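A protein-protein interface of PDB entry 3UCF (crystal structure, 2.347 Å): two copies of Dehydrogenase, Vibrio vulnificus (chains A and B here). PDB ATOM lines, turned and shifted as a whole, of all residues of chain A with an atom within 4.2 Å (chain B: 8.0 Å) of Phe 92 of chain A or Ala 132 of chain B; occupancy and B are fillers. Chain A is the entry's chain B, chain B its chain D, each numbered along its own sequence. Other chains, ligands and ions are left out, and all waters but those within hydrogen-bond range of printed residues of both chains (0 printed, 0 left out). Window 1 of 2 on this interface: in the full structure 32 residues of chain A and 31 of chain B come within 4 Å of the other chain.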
ATOM      1  N   PHE A  88     -20.371  22.907 -11.466  1.00  0.00           N
ATOM      2  CA  PHE A  88     -21.608  22.376 -12.026  1.00  0.00           C
ATOM      3  C   PHE A  88     -22.300  21.471 -11.015  1.00  0.00           C
ATOM      4  O   PHE A  88     -23.516  21.536 -10.842  1.00  0.00           O
ATOM      5  CB  PHE A  88     -21.324  21.589 -13.307  1.00  0.00           C
ATOM      6  CG  PHE A  88     -21.876  22.230 -14.545  1.00  0.00           C
ATOM      7  CD1 PHE A  88     -23.098  21.828 -15.062  1.00  0.00           C
ATOM      8  CD2 PHE A  88     -21.175  23.237 -15.191  1.00  0.00           C
ATOM      9  CE1 PHE A  88     -23.609  22.419 -16.204  1.00  0.00           C
ATOM     10  CE2 PHE A  88     -21.681  23.831 -16.331  1.00  0.00           C
ATOM     11  CZ  PHE A  88     -22.899  23.421 -16.838  1.00  0.00           C
ATOM     12  N   THR A  90     -22.399  21.523  -7.841  1.00  0.00           N
ATOM     13  CA  THR A  90     -23.042  22.225  -6.734  1.00  0.00           C
ATOM     14  C   THR A  90     -24.263  23.025  -7.165  1.00  0.00           C
ATOM     15  O   THR A  90     -25.365  22.775  -6.685  1.00  0.00           O
ATOM     16  CB  THR A  90     -22.058  23.173  -6.019  1.00  0.00           C
ATOM     17  OG1 THR A  90     -21.009  22.405  -5.418  1.00  0.00           O
ATOM     18  CG2 THR A  90     -22.775  23.988  -4.943  1.00  0.00           C
ATOM     19  N   LYS A  91     -24.074  23.988  -8.062  1.00  0.00           N
ATOM     20  CA  LYS A  91     -25.162  24.889  -8.421  1.00  0.00           C
ATOM     21  C   LYS A  91     -26.220  24.239  -9.315  1.00  0.00           C
ATOM     22  O   LYS A  91     -27.414  24.352  -9.038  1.00  0.00           O
ATOM     23  CB  LYS A  91     -24.628  26.161  -9.079  1.00  0.00           C
ATOM     24  CG  LYS A  91     -25.743  27.116  -9.458  1.00  0.00           C
ATOM     25  CD  LYS A  91     -25.274  28.547  -9.653  1.00  0.00           C
ATOM     26  CE  LYS A  91     -26.452  29.437 -10.016  1.00  0.00           C
ATOM     27  NZ  LYS A  91     -26.080  30.873 -10.120  1.00  0.00           N
ATOM     28  N   PHE A  92     -25.797  23.565 -10.379  1.00  0.00           N
ATOM     29  CA  PHE A  92     -26.758  22.972 -11.307  1.00  0.00           C
ATOM     30  C   PHE A  92     -27.314  21.656 -10.781  1.00  0.00           C
ATOM     31  O   PHE A  92     -28.505  21.557 -10.490  1.00  0.00           O
ATOM     32  CB  PHE A  92     -26.150  22.747 -12.693  1.00  0.00           C
ATOM     33  CG  PHE A  92     -27.064  22.008 -13.629  1.00  0.00           C
ATOM     34  CD1 PHE A  92     -28.218  22.610 -14.102  1.00  0.00           C
ATOM     35  CD2 PHE A  92     -26.783  20.708 -14.023  1.00  0.00           C
ATOM     36  CE1 PHE A  92     -29.071  21.936 -14.956  1.00  0.00           C
ATOM     37  CE2 PHE A  92     -27.634  20.029 -14.878  1.00  0.00           C
ATOM     38  CZ  PHE A  92     -28.780  20.644 -15.343  1.00  0.00           C
ATOM     39  N   TRP A  93     -26.456  20.648 -10.666  1.00  0.00           N
ATOM     40  CA  TRP A  93     -26.895  19.332 -10.222  1.00  0.00           C
ATOM     41  C   TRP A  93     -27.450  19.406  -8.805  1.00  0.00           C
ATOM     42  O   TRP A  93     -28.276  18.585  -8.410  1.00  0.00           O
ATOM     43  CB  TRP A  93     -25.749  18.323 -10.311  1.00  0.00           C
ATOM     44  CG  TRP A  93     -25.325  18.055 -11.724  1.00  0.00           C
ATOM     45  CD1 TRP A  93     -24.127  18.365 -12.300  1.00  0.00           C
ATOM     46  CD2 TRP A  93     -26.114  17.435 -12.748  1.00  0.00           C
ATOM     47  NE1 TRP A  93     -24.118  17.970 -13.614  1.00  0.00           N
ATOM     48  CE2 TRP A  93     -25.326  17.398 -13.915  1.00  0.00           C
ATOM     49  CE3 TRP A  93     -27.408  16.906 -12.788  1.00  0.00           C
ATOM     50  CZ2 TRP A  93     -25.790  16.849 -15.113  1.00  0.00           C
ATOM     51  CZ3 TRP A  93     -27.868  16.362 -13.975  1.00  0.00           C
ATOM     52  CH2 TRP A  93     -27.059  16.338 -15.122  1.00  0.00           C
ATOM     53  N   GLY A  94     -26.999  20.401  -8.048  1.00  0.00           N
ATOM     54  CA  GLY A  94     -27.547  20.661  -6.731  1.00  0.00           C
ATOM     55  C   GLY A  94     -29.017  21.021  -6.816  1.00  0.00           C
ATOM     56  O   GLY A  94     -29.835  20.524  -6.042  1.00  0.00           O
ATOM     57  N   ALA A  95     -29.352  21.887  -7.769  1.00  0.00           N
ATOM     58  CA  ALA A  95     -30.733  22.312  -7.976  1.00  0.00           C
ATOM     59  C   ALA A  95     -31.569  21.164  -8.533  1.00  0.00           C
ATOM     60  O   ALA A  95     -32.732  20.995  -8.168  1.00  0.00           O
ATOM     61  CB  ALA A  95     -30.784  23.516  -8.911  1.00  0.00           C
ATOM     62  N   VAL A  96     -30.969  20.376  -9.420  1.00  0.00           N
ATOM     63  CA  VAL A  96     -31.630  19.198  -9.971  1.00  0.00           C
ATOM     64  C   VAL A  96     -31.959  18.213  -8.858  1.00  0.00           C
ATOM     65  O   VAL A  96     -33.081  17.714  -8.767  1.00  0.00           O
ATOM     66  CB  VAL A  96     -30.740  18.494 -11.014  1.00  0.00           C
ATOM     67  CG1 VAL A  96     -31.282  17.109 -11.340  1.00  0.00           C
ATOM     68  CG2 VAL A  96     -30.625  19.342 -12.273  1.00  0.00           C
ATOM     69  N   ALA A 136     -28.423  26.365 -18.198  1.00  0.00           N
ATOM     70  CA  ALA A 136     -28.911  25.021 -17.916  1.00  0.00           C
ATOM     71  C   ALA A 136     -30.047  25.052 -16.894  1.00  0.00           C
ATOM     72  O   ALA A 136     -31.038  24.334 -17.034  1.00  0.00           O
ATOM     73  CB  ALA A 136     -27.772  24.148 -17.415  1.00  0.00           C
ATOM     74  N   ILE A 137     -29.897  25.884 -15.868  1.00  0.00           N
ATOM     75  CA  ILE A 137     -30.908  26.006 -14.823  1.00  0.00           C
ATOM     76  C   ILE A 137     -32.225  26.523 -15.387  1.00  0.00           C
ATOM     77  O   ILE A 137     -33.296  26.030 -15.033  1.00  0.00           O
ATOM     78  CB  ILE A 137     -30.443  26.949 -13.694  1.00  0.00           C
ATOM     79  CG1 ILE A 137     -29.543  26.197 -12.713  1.00  0.00           C
ATOM     80  CG2 ILE A 137     -31.639  27.518 -12.941  1.00  0.00           C
ATOM     81  CD1 ILE A 137     -28.384  27.017 -12.188  1.00  0.00           C
ATOM     82  N   THR A 140     -33.960  23.920 -17.484  1.00  0.00           N
ATOM     83  CA  THR A 140     -34.479  22.870 -16.616  1.00  0.00           C
ATOM     84  C   THR A 140     -35.689  23.376 -15.842  1.00  0.00           C
ATOM     85  O   THR A 140     -36.626  22.626 -15.577  1.00  0.00           O
ATOM     86  CB  THR A 140     -33.413  22.387 -15.616  1.00  0.00           C
ATOM     87  OG1 THR A 140     -32.237  21.972 -16.322  1.00  0.00           O
ATOM     88  CG2 THR A 140     -33.942  21.223 -14.786  1.00  0.00           C
ATOM     89  N   VAL B  81     -29.530  10.556 -11.862  1.00  0.00           N
ATOM     90  CA  VAL B  81     -28.579  11.655 -12.029  1.00  0.00           C
ATOM     91  C   VAL B  81     -27.219  11.197 -12.561  1.00  0.00           C
ATOM     92  O   VAL B  81     -26.529  11.956 -13.244  1.00  0.00           O
ATOM     93  CB  VAL B  81     -28.381  12.428 -10.705  1.00  0.00           C
ATOM     94  CG1 VAL B  81     -27.210  13.401 -10.815  1.00  0.00           C
ATOM     95  CG2 VAL B  81     -29.657  13.166 -10.331  1.00  0.00           C
ATOM     96  N   ALA B  84     -27.551  11.008 -16.233  1.00  0.00           N
ATOM     97  CA  ALA B  84     -27.646  12.381 -16.714  1.00  0.00           C
ATOM     98  C   ALA B  84     -26.262  13.005 -16.821  1.00  0.00           C
ATOM     99  O   ALA B  84     -25.921  13.611 -17.837  1.00  0.00           O
ATOM    100  CB  ALA B  84     -28.525  13.205 -15.785  1.00  0.00           C
ATOM    101  N   LYS B  85     -25.466  12.856 -15.767  1.00  0.00           N
ATOM    102  CA  LYS B  85     -24.111  13.394 -15.748  1.00  0.00           C
ATOM    103  C   LYS B  85     -23.252  12.749 -16.833  1.00  0.00           C
ATOM    104  O   LYS B  85     -22.395  13.401 -17.430  1.00  0.00           O
ATOM    105  CB  LYS B  85     -23.468  13.186 -14.376  1.00  0.00           C
ATOM    106  CG  LYS B  85     -24.045  14.068 -13.280  1.00  0.00           C
ATOM    107  CD  LYS B  85     -23.275  13.900 -11.980  1.00  0.00           C
ATOM    108  CE  LYS B  85     -23.822  14.795 -10.877  1.00  0.00           C
ATOM    109  NZ  LYS B  85     -23.154  14.545  -9.567  1.00  0.00           N
ATOM    110  N   PHE B  88     -24.058  14.460 -19.925  1.00  0.00           N
ATOM    111  CA  PHE B  88     -23.379  15.749 -19.920  1.00  0.00           C
ATOM    112  C   PHE B  88     -21.900  15.592 -20.251  1.00  0.00           C
ATOM    113  O   PHE B  88     -21.328  16.411 -20.968  1.00  0.00           O
ATOM    114  CB  PHE B  88     -23.529  16.422 -18.554  1.00  0.00           C
ATOM    115  CG  PHE B  88     -24.427  17.624 -18.567  1.00  0.00           C
ATOM    116  CD1 PHE B  88     -23.894  18.894 -18.688  1.00  0.00           C
ATOM    117  CD2 PHE B  88     -25.802  17.485 -18.465  1.00  0.00           C
ATOM    118  CE1 PHE B  88     -24.711  20.006 -18.703  1.00  0.00           C
ATOM    119  CE2 PHE B  88     -26.626  18.594 -18.478  1.00  0.00           C
ATOM    120  CZ  PHE B  88     -26.079  19.857 -18.599  1.00  0.00           C
ATOM    121  N   PHE B  92     -21.812  17.844 -23.689  1.00  0.00           N
ATOM    122  CA  PHE B  92     -21.397  19.180 -23.266  1.00  0.00           C
ATOM    123  C   PHE B  92     -19.889  19.254 -23.077  1.00  0.00           C
ATOM    124  O   PHE B  92     -19.193  19.923 -23.841  1.00  0.00           O
ATOM    125  CB  PHE B  92     -22.085  19.624 -21.974  1.00  0.00           C
ATOM    126  CG  PHE B  92     -21.620  20.970 -21.492  1.00  0.00           C
ATOM    127  CD1 PHE B  92     -21.842  22.099 -22.263  1.00  0.00           C
ATOM    128  CD2 PHE B  92     -20.947  21.108 -20.286  1.00  0.00           C
ATOM    129  CE1 PHE B  92     -21.412  23.343 -21.841  1.00  0.00           C
ATOM    130  CE2 PHE B  92     -20.515  22.354 -19.857  1.00  0.00           C
ATOM    131  CZ  PHE B  92     -20.749  23.471 -20.638  1.00  0.00           C
ATOM    132  N   LEU B 119     -34.264  21.343 -28.500  1.00  0.00           N
ATOM    133  CA  LEU B 119     -34.758  21.123 -27.144  1.00  0.00           C
ATOM    134  C   LEU B 119     -34.213  22.149 -26.156  1.00  0.00           C
ATOM    135  O   LEU B 119     -34.685  22.243 -25.023  1.00  0.00           O
ATOM    136  CB  LEU B 119     -34.433  19.707 -26.668  1.00  0.00           C
ATOM    137  CG  LEU B 119     -35.293  18.612 -27.300  1.00  0.00           C
ATOM    138  CD1 LEU B 119     -34.855  17.240 -26.821  1.00  0.00           C
ATOM    139  CD2 LEU B 119     -36.764  18.848 -26.986  1.00  0.00           C
ATOM    140  N   SER B 120     -33.219  22.916 -26.588  1.00  0.00           N
ATOM    141  CA  SER B 120     -32.707  24.009 -25.778  1.00  0.00           C
ATOM    142  C   SER B 120     -33.806  25.035 -25.530  1.00  0.00           C
ATOM    143  O   SER B 120     -33.815  25.703 -24.495  1.00  0.00           O
ATOM    144  CB  SER B 120     -31.520  24.679 -26.470  1.00  0.00           C
ATOM    145  OG  SER B 120     -31.883  25.157 -27.752  1.00  0.00           O
ATOM    146  N   ARG B 121     -34.733  25.154 -26.477  1.00  0.00           N
ATOM    147  CA  ARG B 121     -35.773  26.178 -26.405  1.00  0.00           C
ATOM    148  C   ARG B 121     -37.198  25.638 -26.554  1.00  0.00           C
ATOM    149  O   ARG B 121     -38.152  26.293 -26.134  1.00  0.00           O
ATOM    150  CB  ARG B 121     -35.509  27.269 -27.445  1.00  0.00           C
ATOM    151  CG  ARG B 121     -34.446  28.264 -27.016  1.00  0.00           C
ATOM    152  CD  ARG B 121     -33.259  28.236 -27.951  1.00  0.00           C
ATOM    153  NE  ARG B 121     -33.638  28.602 -29.310  1.00  0.00           N
ATOM    154  CZ  ARG B 121     -33.088  28.094 -30.407  1.00  0.00           C
ATOM    155  NH1 ARG B 121     -32.126  27.183 -30.321  1.00  0.00           N
ATOM    156  NH2 ARG B 121     -33.506  28.494 -31.598  1.00  0.00           N
ATOM    157  N   THR B 127     -37.332  15.609 -21.259  1.00  0.00           N
ATOM    158  CA  THR B 127     -36.107  15.945 -21.983  1.00  0.00           C
ATOM    159  C   THR B 127     -35.228  16.994 -21.303  1.00  0.00           C
ATOM    160  O   THR B 127     -34.518  17.737 -21.981  1.00  0.00           O
ATOM    161  CB  THR B 127     -36.432  16.471 -23.395  1.00  0.00           C
ATOM    162  OG1 THR B 127     -37.086  17.743 -23.295  1.00  0.00           O
ATOM    163  CG2 THR B 127     -37.325  15.496 -24.143  1.00  0.00           C
ATOM    164  N   TYR B 128     -35.258  17.058 -19.977  1.00  0.00           N
ATOM    165  CA  TYR B 128     -34.503  18.087 -19.259  1.00  0.00           C
ATOM    166  C   TYR B 128     -32.991  17.965 -19.457  1.00  0.00           C
ATOM    167  O   TYR B 128     -32.285  18.972 -19.488  1.00  0.00           O
ATOM    168  CB  TYR B 128     -34.843  18.072 -17.764  1.00  0.00           C
ATOM    169  CG  TYR B 128     -33.909  17.253 -16.901  1.00  0.00           C
ATOM    170  CD1 TYR B 128     -32.701  17.784 -16.452  1.00  0.00           C
ATOM    171  CD2 TYR B 128     -34.246  15.961 -16.507  1.00  0.00           C
ATOM    172  CE1 TYR B 128     -31.849  17.047 -15.653  1.00  0.00           C
ATOM    173  CE2 TYR B 128     -33.398  15.213 -15.704  1.00  0.00           C
ATOM    174  CZ  TYR B 128     -32.201  15.763 -15.282  1.00  0.00           C
ATOM    175  OH  TYR B 128     -31.361  15.030 -14.482  1.00  0.00           O
ATOM    176  N   VAL B 129     -32.495  16.738 -19.593  1.00  0.00           N
ATOM    177  CA  VAL B 129     -31.060  16.512 -19.757  1.00  0.00           C
ATOM    178  C   VAL B 129     -30.573  17.049 -21.100  1.00  0.00           C
ATOM    179  O   VAL B 129     -29.552  17.733 -21.173  1.00  0.00           O
ATOM    180  CB  VAL B 129     -30.705  15.016 -19.648  1.00  0.00           C
ATOM    181  CG1 VAL B 129     -29.249  14.785 -20.027  1.00  0.00           C
ATOM    182  CG2 VAL B 129     -30.980  14.503 -18.241  1.00  0.00           C
ATOM    183  N   LYS B 130     -31.306  16.733 -22.161  1.00  0.00           N
ATOM    184  CA  LYS B 130     -30.951  17.192 -23.500  1.00  0.00           C
ATOM    185  C   LYS B 130     -31.123  18.705 -23.606  1.00  0.00           C
ATOM    186  O   LYS B 130     -30.313  19.396 -24.227  1.00  0.00           O
ATOM    187  CB  LYS B 130     -31.818  16.493 -24.547  1.00  0.00           C
ATOM    188  N   ALA B 131     -32.186  19.211 -22.992  1.00  0.00           N
ATOM    189  CA  ALA B 131     -32.465  20.642 -22.990  1.00  0.00           C
ATOM    190  C   ALA B 131     -31.377  21.407 -22.243  1.00  0.00           C
ATOM    191  O   ALA B 131     -30.902  22.446 -22.702  1.00  0.00           O
ATOM    192  CB  ALA B 131     -33.823  20.912 -22.359  1.00  0.00           C
ATOM    193  N   ALA B 132     -30.986  20.885 -21.084  1.00  0.00           N
ATOM    194  CA  ALA B 132     -29.960  21.521 -20.267  1.00  0.00           C
ATOM    195  C   ALA B 132     -28.622  21.520 -20.999  1.00  0.00           C
ATOM    196  O   ALA B 132     -27.930  22.538 -21.051  1.00  0.00           O
ATOM    197  CB  ALA B 132     -29.833  20.809 -18.929  1.00  0.00           C
ATOM    198  N   ILE B 133     -28.264  20.370 -21.563  1.00  0.00           N
ATOM    199  CA  ILE B 133     -27.034  20.244 -22.337  1.00  0.00           C
ATOM    200  C   ILE B 133     -26.998  21.269 -23.465  1.00  0.00           C
ATOM    201  O   ILE B 133     -26.037  22.025 -23.600  1.00  0.00           O
ATOM    202  CB  ILE B 133     -26.899  18.832 -22.949  1.00  0.00           C
ATOM    203  CG1 ILE B 133     -26.518  17.809 -21.877  1.00  0.00           C
ATOM    204  CG2 ILE B 133     -25.847  18.821 -24.048  1.00  0.00           C
ATOM    205  CD1 ILE B 133     -26.527  16.381 -22.383  1.00  0.00           C
ATOM    206  N   ASN B 134     -28.057  21.287 -24.269  1.00  0.00           N
ATOM    207  CA  ASN B 134     -28.125  22.153 -25.443  1.00  0.00           C
ATOM    208  C   ASN B 134     -28.106  23.638 -25.093  1.00  0.00           C
ATOM    209  O   ASN B 134     -27.490  24.440 -25.795  1.00  0.00           O
ATOM    210  CB  ASN B 134     -29.371  21.825 -26.269  1.00  0.00           C
ATOM    211  CG  ASN B 134     -29.257  20.494 -26.995  1.00  0.00           C
ATOM    212  OD1 ASN B 134     -28.155  20.003 -27.240  1.00  0.00           O
ATOM    213  ND2 ASN B 134     -30.394  19.911 -27.351  1.00  0.00           N
ATOM    214  N   ALA B 135     -28.787  24.001 -24.012  1.00  0.00           N
ATOM    215  CA  ALA B 135     -28.796  25.385 -23.548  1.00  0.00           C
ATOM    216  C   ALA B 135     -27.395  25.801 -23.115  1.00  0.00           C
ATOM    217  O   ALA B 135     -26.957  26.920 -23.384  1.00  0.00           O
ATOM    218  CB  ALA B 135     -29.778  25.555 -22.399  1.00  0.00           C
ATOM    219  N   ALA B 136     -26.697  24.893 -22.441  1.00  0.00           N
ATOM    220  CA  ALA B 136     -25.336  25.155 -21.989  1.00  0.00           C
ATOM    221  C   ALA B 136     -24.386  25.304 -23.176  1.00  0.00           C
ATOM    222  O   ALA B 136     -23.520  26.180 -23.180  1.00  0.00           O
ATOM    223  CB  ALA B 136     -24.866  24.044 -21.066  1.00  0.00           C
ATOM    224  N   ILE B 137     -24.552  24.445 -24.177  1.00  0.00           N
ATOM    225  CA  ILE B 137     -23.731  24.498 -25.382  1.00  0.00           C
ATOM    226  C   ILE B 137     -23.878  25.838 -26.093  1.00  0.00           C
ATOM    227  O   ILE B 137     -22.896  26.409 -26.565  1.00  0.00           O
ATOM    228  CB  ILE B 137     -24.113  23.373 -26.364  1.00  0.00           C
ATOM    229  CG1 ILE B 137     -23.517  22.042 -25.903  1.00  0.00           C
ATOM    230  CG2 ILE B 137     -23.614  23.695 -27.765  1.00  0.00           C
ATOM    231  CD1 ILE B 137     -24.300  20.830 -26.361  1.00  0.00           C
ATOM    232  N   GLU B 138     -25.110  26.334 -26.169  1.00  0.00           N
ATOM    233  CA  GLU B 138     -25.399  27.577 -26.879  1.00  0.00           C
ATOM    234  C   GLU B 138     -24.859  28.801 -26.145  1.00  0.00           C
ATOM    235  O   GLU B 138     -24.454  29.779 -26.775  1.00  0.00           O
ATOM    236  CB  GLU B 138     -26.904  27.716 -27.105  1.00  0.00           C
ATOM    237  CG  GLU B 138     -27.453  26.741 -28.133  1.00  0.00           C
ATOM    238  CD  GLU B 138     -28.953  26.855 -28.305  1.00  0.00           C
ATOM    239  OE1 GLU B 138     -29.545  27.806 -27.753  1.00  0.00           O
ATOM    240  OE2 GLU B 138     -29.538  25.994 -28.993  1.00  0.00           O
ATOM    241  N   ALA B 139     -24.856  28.746 -24.818  1.00  0.00           N
ATOM    242  CA  ALA B 139     -24.278  29.820 -24.016  1.00  0.00           C
ATOM    243  C   ALA B 139     -22.761  29.803 -24.144  1.00  0.00           C
ATOM    244  O   ALA B 139     -22.122  30.850 -24.252  1.00  0.00           O
ATOM    245  CB  ALA B 139     -24.688  29.680 -22.556  1.00  0.00           C
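The backbone carbonyl oxygen (O) of Ala 136 of chain A is in hydrogen-bond range of the side-chain hydroxyl (OG1) of Thr 140 of chain A, at 2.7 Å.
O of Phe 88 of chain A lies within hydrogen-bond range of N of Trp 93 of chain A, 3.1 Å away.
Phe 88 of chain B touches Phe 88 of chain A.
CZ of Phe 88 of chain A touches CE2 of Phe 92 of chain B, at 3.99 Å.
CB of Ala 132 of chain B touches CZ of Phe 92 of chain A, at 3.7 Å.
CH2 of Trp 93 of chain A touches CB of Ala 84 of chain B, at 3.5 Å.
Lys 85 of chain B touches Trp 93 of chain A (CG to CE2, 3.6 Å).
Trp 93 of chain A touches Phe 88 of chain B (CZ2 to CD2, 3.4 Å).
Tyr 128 of chain B touches Trp 93 of chain A (OH to CZ3, 3.8 Å).
Val 96 of chain A touches Tyr 128 of chain B.
Ala 132 of chain B touches Ala 136 of chain A (O to CB, 3.98 Å).
Ala 132 of chain B touches Thr 140 of chain A (CB to OG1, 3.7 Å).
Of the printed residues of chain B, Phe 92 of chain A touches Ala 132.
Of the printed residues of chain A, Lys 85 of chain B touches Trp 93 (3.6 Å).
Printed residues of chain A within 4 Å of Phe 88 of chain B: Phe 88 and Trp 93.
Ala 132 of chain B touches just these residues of chain A: Phe 92, Ala 136 and Thr 140.
Glu 138 of chain B touches none of the printed residues of chain A.
The nearest printed residue of chain B that does not touch Phe 92 of chain A is Phe 88 of chain B (4.004 Å).
The nearest printed residue of chain A that does not touch Ala 132 of chain B is Ile 137 of chain A (5.9 Å).
The nearest printed residue of chain A that does not touch Ala 84 of chain B is Val 96 of chain A (6.5 Å).
Among the printed residues, 10 pairs touch across the chains.
Phe 88 of chain A touches its own counterpart, Phe 88 of chain B.
Phe 88 of chain A touches Phe 92 of chain B, but with the chains exchanged Phe 92 of chain A does not touch Phe 88 of chain B (4.004 Å).
4 positions are printed for both chains.
Of the 10 pairs that touch across the chains among the printed residues, 1 has its exchanged pair printed and touching as well.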
